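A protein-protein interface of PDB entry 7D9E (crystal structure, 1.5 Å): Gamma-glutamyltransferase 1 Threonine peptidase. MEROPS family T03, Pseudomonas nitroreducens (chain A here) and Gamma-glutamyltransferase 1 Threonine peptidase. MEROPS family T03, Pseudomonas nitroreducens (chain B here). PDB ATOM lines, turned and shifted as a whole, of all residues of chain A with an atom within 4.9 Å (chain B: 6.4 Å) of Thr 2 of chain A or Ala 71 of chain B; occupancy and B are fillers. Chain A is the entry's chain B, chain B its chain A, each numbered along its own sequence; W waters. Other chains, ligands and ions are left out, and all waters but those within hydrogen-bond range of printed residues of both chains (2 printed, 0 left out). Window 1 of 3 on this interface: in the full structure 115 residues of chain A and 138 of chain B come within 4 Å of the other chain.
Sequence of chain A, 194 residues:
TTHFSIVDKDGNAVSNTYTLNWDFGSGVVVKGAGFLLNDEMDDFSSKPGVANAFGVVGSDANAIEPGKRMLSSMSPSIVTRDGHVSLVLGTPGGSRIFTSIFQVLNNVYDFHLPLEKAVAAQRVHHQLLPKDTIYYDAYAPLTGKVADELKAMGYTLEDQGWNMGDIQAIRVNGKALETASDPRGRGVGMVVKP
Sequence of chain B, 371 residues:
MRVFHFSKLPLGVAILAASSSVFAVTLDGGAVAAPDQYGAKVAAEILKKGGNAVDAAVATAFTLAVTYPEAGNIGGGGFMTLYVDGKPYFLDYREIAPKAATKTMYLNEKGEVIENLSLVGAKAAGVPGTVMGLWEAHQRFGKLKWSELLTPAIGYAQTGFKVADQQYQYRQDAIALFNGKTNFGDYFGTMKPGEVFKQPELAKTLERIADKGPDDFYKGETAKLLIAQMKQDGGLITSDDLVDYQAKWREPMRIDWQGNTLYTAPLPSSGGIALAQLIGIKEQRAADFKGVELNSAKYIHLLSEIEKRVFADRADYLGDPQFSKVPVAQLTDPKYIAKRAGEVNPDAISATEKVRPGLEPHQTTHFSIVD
O of Gly 77 of chain B is in hydrogen-bond range of N of Thr 19 of chain A, 2.9 Å away.
The side-chain amide nitrogen of Asn 73 of chain B is in hydrogen-bond range of the backbone carbonyl oxygen of Thr 19 of chain A (3.2 Å).
OG1 of Thr 19 of chain A lies within hydrogen-bond range of N of Thr 1 of chain A (3.0 Å).
The backbone carbonyl oxygen (O) of Ala 71 of chain B is in hydrogen-bond range of the side-chain amide nitrogen (ND2) of Asn 73 of chain B (2.9 Å).
O of Phe 4 of chain A lies within hydrogen-bond range of N of Asn 16 of chain A, at 2.9 Å.
A ring nitrogen (ND1) of His 3 of chain A lies within hydrogen-bond range of the side-chain hydroxyl (OG1) of Thr 17 of chain A (2.7 Å).
The backbone carbonyl oxygen (O) of Tyr 18 of chain A lies within hydrogen-bond range of the backbone NH (N) of Thr 2 of chain A (2.9 Å).
A ring nitrogen (ND1) of His 3 of chain A sits at hydrogen-bond distance from the backbone carbonyl oxygen (O) of Asn 16 of chain A (3.1 Å).
Among the printed residues, pairs that only touch across the chains: Thr 2 of chain A with Pro 35 of chain B (3.1 Å), Tyr 18 of chain A with Leu 64 of chain B (3.3 Å), Tyr 18 of chain A with Gly 77 of chain B (3.3 Å), His 3 of chain A with Pro 35 of chain B (3.4 Å), Thr 1 of chain A with Ala 71 of chain B (3.4 Å), Tyr 18 of chain A with Gly 72 of chain B (3.4 Å), Leu 20 of chain A with Pro 69 of chain B (3.4 Å), Leu 20 of chain A with Asn 73 of chain B (3.6 Å), Tyr 18 of chain A with Asn 73 of chain B (3.6 Å), Thr 19 of chain A with Ala 71 of chain B (3.6 Å), Tyr 18 of chain A with Ala 65 of chain B (3.6 Å), Phe 4 of chain A with Leu 64 of chain B (3.7 Å), Thr 2 of chain A with Ala 71 of chain B (3.7 Å), Leu 20 of chain A with Ala 71 of chain B (3.8 Å), Thr 2 of chain A with Tyr 68 of chain B (3.8 Å), Phe 4 of chain A with Pro 35 of chain B (3.9 Å) and Thr 2 of chain A with Gly 72 of chain B (3.9 Å).
Printed residues of chain B within 4 Å of Thr 2 of chain A: Pro 35, Tyr 68, Ala 71 and Gly 72.
Ala 71 of chain B touches four residues of chain A.
Printed residues of chain A within 4 Å of Pro 69 of chain B: Leu 20.
Printed residues of chain A within 4 Å of Gly 72 of chain B: Thr 2 and Tyr 18.
Printed residues of chain B within 4 Å of Leu 20 of chain A: Pro 69 (3.4 Å), Ala 71 (3.8 Å) and Asn 73 (3.6 Å).
Printed residues of chain A within 4 Å of Pro 35 of chain B: Thr 2, His 3 and Phe 4.
Pro 92 of chain A touches none of the printed residues of chain B.
The nearest printed residue of chain A that does not touch Ala 71 of chain B is Tyr 18 of chain A (4.1 Å).
The nearest printed residue of chain A that does not touch Leu 64 of chain B is Thr 2 of chain A (4.7 Å).
Of the 12 printed residues of chain B, 9 touch a printed residue of chain A.
Of the 10 printed residues of chain A, 7 touch a printed residue of chain B.
Hydrophobic or aromatic side chains of chain A that line the printed part of chain B: Phe 4, Tyr 18 and Leu 20.
Water W1 lies within hydrogen-bond range of the side-chain hydroxyl of Thr 2 of chain A (2.8 Å) and the side-chain hydroxyl of Tyr 68 of chain B (3.0 Å).
Water W2 lies within hydrogen-bond range of O of Glu 70 of chain B (2.9 Å), N of Thr 1 of chain A (3.0 Å), N of Leu 20 of chain A (3.0 Å) and OG1 of Thr 19 of chain A (3.2 Å).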
ATOM      1  N   THR A   1      20.262  22.513  13.724  1.00  0.00           N
ATOM      2  CA  THR A   1      20.641  21.253  14.334  1.00  0.00           C
ATOM      3  C   THR A   1      20.425  21.239  15.845  1.00  0.00           C
ATOM      4  O   THR A   1      20.556  22.265  16.531  1.00  0.00           O
ATOM      5  CB  THR A   1      22.137  20.943  14.080  1.00  0.00           C
ATOM      6  OG1 THR A   1      22.458  21.055  12.678  1.00  0.00           O
ATOM      7  CG2 THR A   1      22.519  19.574  14.594  1.00  0.00           C
ATOM      8  N   THR A   2      20.093  20.062  16.362  1.00  0.00           N
ATOM      9  CA  THR A   2      20.205  19.793  17.793  1.00  0.00           C
ATOM     10  C   THR A   2      20.654  18.350  17.958  1.00  0.00           C
ATOM     11  O   THR A   2      20.641  17.564  17.010  1.00  0.00           O
ATOM     12  CB  THR A   2      18.908  20.100  18.537  1.00  0.00           C
ATOM     13  OG1 THR A   2      19.158  20.103  19.938  1.00  0.00           O
ATOM     14  CG2 THR A   2      17.796  19.104  18.233  1.00  0.00           C
ATOM     15  N   HIS A   3      21.083  18.020  19.170  1.00  0.00           N
ATOM     16  CA  HIS A   3      21.616  16.713  19.464  1.00  0.00           C
ATOM     17  C   HIS A   3      21.091  16.261  20.817  1.00  0.00           C
ATOM     18  O   HIS A   3      20.998  17.059  21.751  1.00  0.00           O
ATOM     19  CB  HIS A   3      23.167  16.759  19.548  1.00  0.00           C
ATOM     20  CG  HIS A   3      23.755  15.421  19.823  1.00  0.00           C
ATOM     21  ND1 HIS A   3      23.942  14.481  18.835  1.00  0.00           N
ATOM     22  CD2 HIS A   3      24.129  14.834  20.985  1.00  0.00           C
ATOM     23  CE1 HIS A   3      24.386  13.361  19.378  1.00  0.00           C
ATOM     24  NE2 HIS A   3      24.514  13.555  20.684  1.00  0.00           N
ATOM     25  N   PHE A   4      20.844  14.959  20.956  1.00  0.00           N
ATOM     26  CA  PHE A   4      20.624  14.368  22.272  1.00  0.00           C
ATOM     27  C   PHE A   4      21.350  13.035  22.366  1.00  0.00           C
ATOM     28  O   PHE A   4      21.630  12.364  21.361  1.00  0.00           O
ATOM     29  CB  PHE A   4      19.130  14.233  22.619  1.00  0.00           C
ATOM     30  CG  PHE A   4      18.338  13.350  21.707  1.00  0.00           C
ATOM     31  CD1 PHE A   4      18.288  11.971  21.903  1.00  0.00           C
ATOM     32  CD2 PHE A   4      17.596  13.887  20.683  1.00  0.00           C
ATOM     33  CE1 PHE A   4      17.534  11.164  21.094  1.00  0.00           C
ATOM     34  CE2 PHE A   4      16.844  13.074  19.848  1.00  0.00           C
ATOM     35  CZ  PHE A   4      16.814  11.725  20.053  1.00  0.00           C
ATOM     36  N   ASN A  16      22.017  11.016  18.767  1.00  0.00           N
ATOM     37  CA  ASN A  16      21.166  11.408  17.643  1.00  0.00           C
ATOM     38  C   ASN A  16      21.310  12.890  17.359  1.00  0.00           C
ATOM     39  O   ASN A  16      20.995  13.718  18.221  1.00  0.00           O
ATOM     40  CB  ASN A  16      19.707  11.101  17.957  1.00  0.00           C
ATOM     41  CG  ASN A  16      18.838  11.270  16.768  1.00  0.00           C
ATOM     42  OD1 ASN A  16      18.765  10.390  15.928  1.00  0.00           O
ATOM     43  ND2 ASN A  16      18.207  12.435  16.658  1.00  0.00           N
ATOM     44  N   THR A  17      21.746  13.222  16.135  1.00  0.00           N
ATOM     45  CA  THR A  17      21.843  14.605  15.681  1.00  0.00           C
ATOM     46  C   THR A  17      20.861  14.754  14.533  1.00  0.00           C
ATOM     47  O   THR A  17      20.897  13.968  13.579  1.00  0.00           O
ATOM     48  CB  THR A  17      23.260  14.950  15.180  1.00  0.00           C
ATOM     49  OG1 THR A  17      24.253  14.568  16.145  1.00  0.00           O
ATOM     50  CG2 THR A  17      23.381  16.431  14.975  1.00  0.00           C
ATOM     51  N   TYR A  18      19.993  15.763  14.607  1.00  0.00           N
ATOM     52  CA  TYR A  18      19.041  15.980  13.522  1.00  0.00           C
ATOM     53  C   TYR A  18      18.756  17.468  13.397  1.00  0.00           C
ATOM     54  O   TYR A  18      19.101  18.267  14.269  1.00  0.00           O
ATOM     55  CB  TYR A  18      17.826  15.035  13.616  1.00  0.00           C
ATOM     56  CG  TYR A  18      16.757  15.315  14.645  1.00  0.00           C
ATOM     57  CD1 TYR A  18      17.002  16.080  15.772  1.00  0.00           C
ATOM     58  CD2 TYR A  18      15.487  14.769  14.498  1.00  0.00           C
ATOM     59  CE1 TYR A  18      16.002  16.321  16.714  1.00  0.00           C
ATOM     60  CE2 TYR A  18      14.480  15.012  15.425  1.00  0.00           C
ATOM     61  CZ  TYR A  18      14.751  15.784  16.533  1.00  0.00           C
ATOM     62  OH  TYR A  18      13.773  16.036  17.467  1.00  0.00           O
ATOM     63  N   THR A  19      18.126  17.847  12.287  1.00  0.00           N
ATOM     64  CA  THR A  19      18.174  19.238  11.868  1.00  0.00           C
ATOM     65  C   THR A  19      17.168  19.579  10.791  1.00  0.00           C
ATOM     66  O   THR A  19      16.700  18.713  10.047  1.00  0.00           O
ATOM     67  CB  THR A  19      19.601  19.576  11.353  1.00  0.00           C
ATOM     68  OG1 THR A  19      19.765  20.995  11.243  1.00  0.00           O
ATOM     69  CG2 THR A  19      19.928  18.909  10.030  1.00  0.00           C
ATOM     70  N   LEU A  20      16.883  20.887  10.699  1.00  0.00           N
ATOM     71  CA  LEU A  20      16.263  21.532   9.543  1.00  0.00           C
ATOM     72  C   LEU A  20      17.285  22.288   8.697  1.00  0.00           C
ATOM     73  O   LEU A  20      16.931  22.841   7.657  1.00  0.00           O
ATOM     74  CB  LEU A  20      15.224  22.528  10.020  1.00  0.00           C
ATOM     75  CG  LEU A  20      13.973  21.951  10.666  1.00  0.00           C
ATOM     76  CD1 LEU A  20      13.147  23.120  11.169  1.00  0.00           C
ATOM     77  CD2 LEU A  20      13.180  21.106   9.718  1.00  0.00           C
ATOM     78  N   PRO A  92      25.153  20.466  17.756  1.00  0.00           N
ATOM     79  CA  PRO A  92      24.919  21.305  16.575  1.00  0.00           C
ATOM     80  C   PRO A  92      26.136  22.175  16.288  1.00  0.00           C
ATOM     81  O   PRO A  92      27.127  22.173  17.019  1.00  0.00           O
ATOM     82  CB  PRO A  92      23.757  22.184  17.013  1.00  0.00           C
ATOM     83  CG  PRO A  92      23.937  22.336  18.520  1.00  0.00           C
ATOM     84  CD  PRO A  92      24.425  20.984  18.938  1.00  0.00           C
ATOM     85  N   ALA B  34      19.711  16.035  27.034  1.00  0.00           N
ATOM     86  CA  ALA B  34      18.831  16.548  26.005  1.00  0.00           C
ATOM     87  C   ALA B  34      18.976  18.053  25.889  1.00  0.00           C
ATOM     88  O   ALA B  34      19.366  18.730  26.844  1.00  0.00           O
ATOM     89  CB  ALA B  34      17.369  16.192  26.319  1.00  0.00           C
ATOM     90  N   PRO B  35      18.635  18.617  24.730  1.00  0.00           N
ATOM     91  CA  PRO B  35      18.825  20.066  24.548  1.00  0.00           C
ATOM     92  C   PRO B  35      17.764  20.924  25.187  1.00  0.00           C
ATOM     93  O   PRO B  35      17.919  22.156  25.183  1.00  0.00           O
ATOM     94  CB  PRO B  35      18.822  20.229  23.033  1.00  0.00           C
ATOM     95  CG  PRO B  35      17.906  19.126  22.554  1.00  0.00           C
ATOM     96  CD  PRO B  35      18.261  17.950  23.467  1.00  0.00           C
ATOM     97  N   ASP B  36      16.710  20.336  25.751  1.00  0.00           N
ATOM     98  CA  ASP B  36      15.797  21.093  26.594  1.00  0.00           C
ATOM     99  C   ASP B  36      15.197  20.187  27.658  1.00  0.00           C
ATOM    100  O   ASP B  36      15.411  18.969  27.665  1.00  0.00           O
ATOM    101  CB  ASP B  36      14.733  21.870  25.800  1.00  0.00           C
ATOM    102  CG  ASP B  36      13.630  20.994  25.198  1.00  0.00           C
ATOM    103  OD1 ASP B  36      13.445  19.827  25.624  1.00  0.00           O
ATOM    104  OD2 ASP B  36      12.902  21.506  24.313  1.00  0.00           O
ATOM    105  N   LEU B  64      11.044  16.787  20.776  1.00  0.00           N
ATOM    106  CA  LEU B  64      11.769  17.974  20.342  1.00  0.00           C
ATOM    107  C   LEU B  64      11.258  18.527  19.015  1.00  0.00           C
ATOM    108  O   LEU B  64      11.451  19.719  18.741  1.00  0.00           O
ATOM    109  CB  LEU B  64      13.259  17.663  20.270  1.00  0.00           C
ATOM    110  CG  LEU B  64      13.907  17.262  21.597  1.00  0.00           C
ATOM    111  CD1 LEU B  64      15.332  16.720  21.400  1.00  0.00           C
ATOM    112  CD2 LEU B  64      13.921  18.440  22.555  1.00  0.00           C
ATOM    113  N   ALA B  65      10.611  17.698  18.187  1.00  0.00           N
ATOM    114  CA  ALA B  65       9.947  18.186  16.988  1.00  0.00           C
ATOM    115  C   ALA B  65       8.803  19.131  17.330  1.00  0.00           C
ATOM    116  O   ALA B  65       8.380  19.927  16.475  1.00  0.00           O
ATOM    117  CB  ALA B  65       9.448  16.997  16.176  1.00  0.00           C
ATOM    118  N   TYR B  68      11.269  22.070  20.224  1.00  0.00           N
ATOM    119  CA  TYR B  68      12.536  22.718  19.925  1.00  0.00           C
ATOM    120  C   TYR B  68      12.407  22.867  18.364  1.00  0.00           C
ATOM    121  O   TYR B  68      13.275  22.395  17.623  1.00  0.00           O
ATOM    122  CB  TYR B  68      13.643  21.762  20.211  1.00  0.00           C
ATOM    123  CG  TYR B  68      15.025  22.337  20.466  1.00  0.00           C
ATOM    124  CD1 TYR B  68      15.351  22.710  21.751  1.00  0.00           C
ATOM    125  CD2 TYR B  68      15.885  22.708  19.469  1.00  0.00           C
ATOM    126  CE1 TYR B  68      16.577  23.230  22.068  1.00  0.00           C
ATOM    127  CE2 TYR B  68      17.123  23.295  19.774  1.00  0.00           C
ATOM    128  CZ  TYR B  68      17.442  23.555  21.084  1.00  0.00           C
ATOM    129  OH  TYR B  68      18.635  24.143  21.458  1.00  0.00           O
ATOM    130  N   PRO B  69      11.337  23.502  17.861  1.00  0.00           N
ATOM    131  CA  PRO B  69      11.082  23.497  16.403  1.00  0.00           C
ATOM    132  C   PRO B  69      12.140  24.207  15.561  1.00  0.00           C
ATOM    133  O   PRO B  69      12.135  24.061  14.316  1.00  0.00           O
ATOM    134  CB  PRO B  69       9.734  24.227  16.279  1.00  0.00           C
ATOM    135  CG  PRO B  69       9.640  25.057  17.515  1.00  0.00           C
ATOM    136  CD  PRO B  69      10.277  24.202  18.592  1.00  0.00           C
ATOM    137  N   GLU B  70      13.028  24.982  16.173  1.00  0.00           N
ATOM    138  CA  GLU B  70      14.124  25.554  15.407  1.00  0.00           C
ATOM    139  C   GLU B  70      15.011  24.475  14.804  1.00  0.00           C
ATOM    140  O   GLU B  70      15.712  24.742  13.817  1.00  0.00           O
ATOM    141  CB  GLU B  70      14.923  26.525  16.273  1.00  0.00           C
ATOM    142  CG  GLU B  70      15.527  25.949  17.538  1.00  0.00           C
ATOM    143  CD  GLU B  70      14.647  26.080  18.778  1.00  0.00           C
ATOM    144  OE1 GLU B  70      13.430  25.770  18.698  1.00  0.00           O
ATOM    145  OE2 GLU B  70      15.185  26.510  19.831  1.00  0.00           O
ATOM    146  N   ALA B  71      14.999  23.263  15.366  1.00  0.00           N
ATOM    147  CA  ALA B  71      15.915  22.221  14.930  1.00  0.00           C
ATOM    148  C   ALA B  71      15.335  20.816  15.039  1.00  0.00           C
ATOM    149  O   ALA B  71      15.427  20.041  14.085  1.00  0.00           O
ATOM    150  CB  ALA B  71      17.229  22.315  15.709  1.00  0.00           C
ATOM    151  N   GLY B  72      14.743  20.470  16.182  1.00  0.00           N
ATOM    152  CA  GLY B  72      13.977  19.239  16.246  1.00  0.00           C
ATOM    153  C   GLY B  72      12.858  19.285  15.231  1.00  0.00           C
ATOM    154  O   GLY B  72      12.313  20.353  14.945  1.00  0.00           O
ATOM    155  N   ASN B  73      12.528  18.135  14.656  1.00  0.00           N
ATOM    156  CA  ASN B  73      11.741  18.222  13.440  1.00  0.00           C
ATOM    157  C   ASN B  73      11.135  16.890  13.044  1.00  0.00           C
ATOM    158  O   ASN B  73      11.648  15.824  13.385  1.00  0.00           O
ATOM    159  CB  ASN B  73      12.643  18.685  12.287  1.00  0.00           C
ATOM    160  CG  ASN B  73      13.648  17.632  11.892  1.00  0.00           C
ATOM    161  OD1 ASN B  73      13.353  16.746  11.079  1.00  0.00           O
ATOM    162  ND2 ASN B  73      14.856  17.722  12.455  1.00  0.00           N
ATOM    163  N   GLY B  77      15.959  16.048   8.654  1.00  0.00           N
ATOM    164  CA  GLY B  77      16.635  14.761   8.601  1.00  0.00           C
ATOM    165  C   GLY B  77      17.762  14.729   9.608  1.00  0.00           C
ATOM    166  O   GLY B  77      17.965  15.681  10.364  1.00  0.00           O
HETATM  167  O   HOH W   1      20.750  22.290  20.489  1.00  0.00           O
HETATM  168  O   HOH W   2      17.745  23.291  12.342  1.00  0.00           O
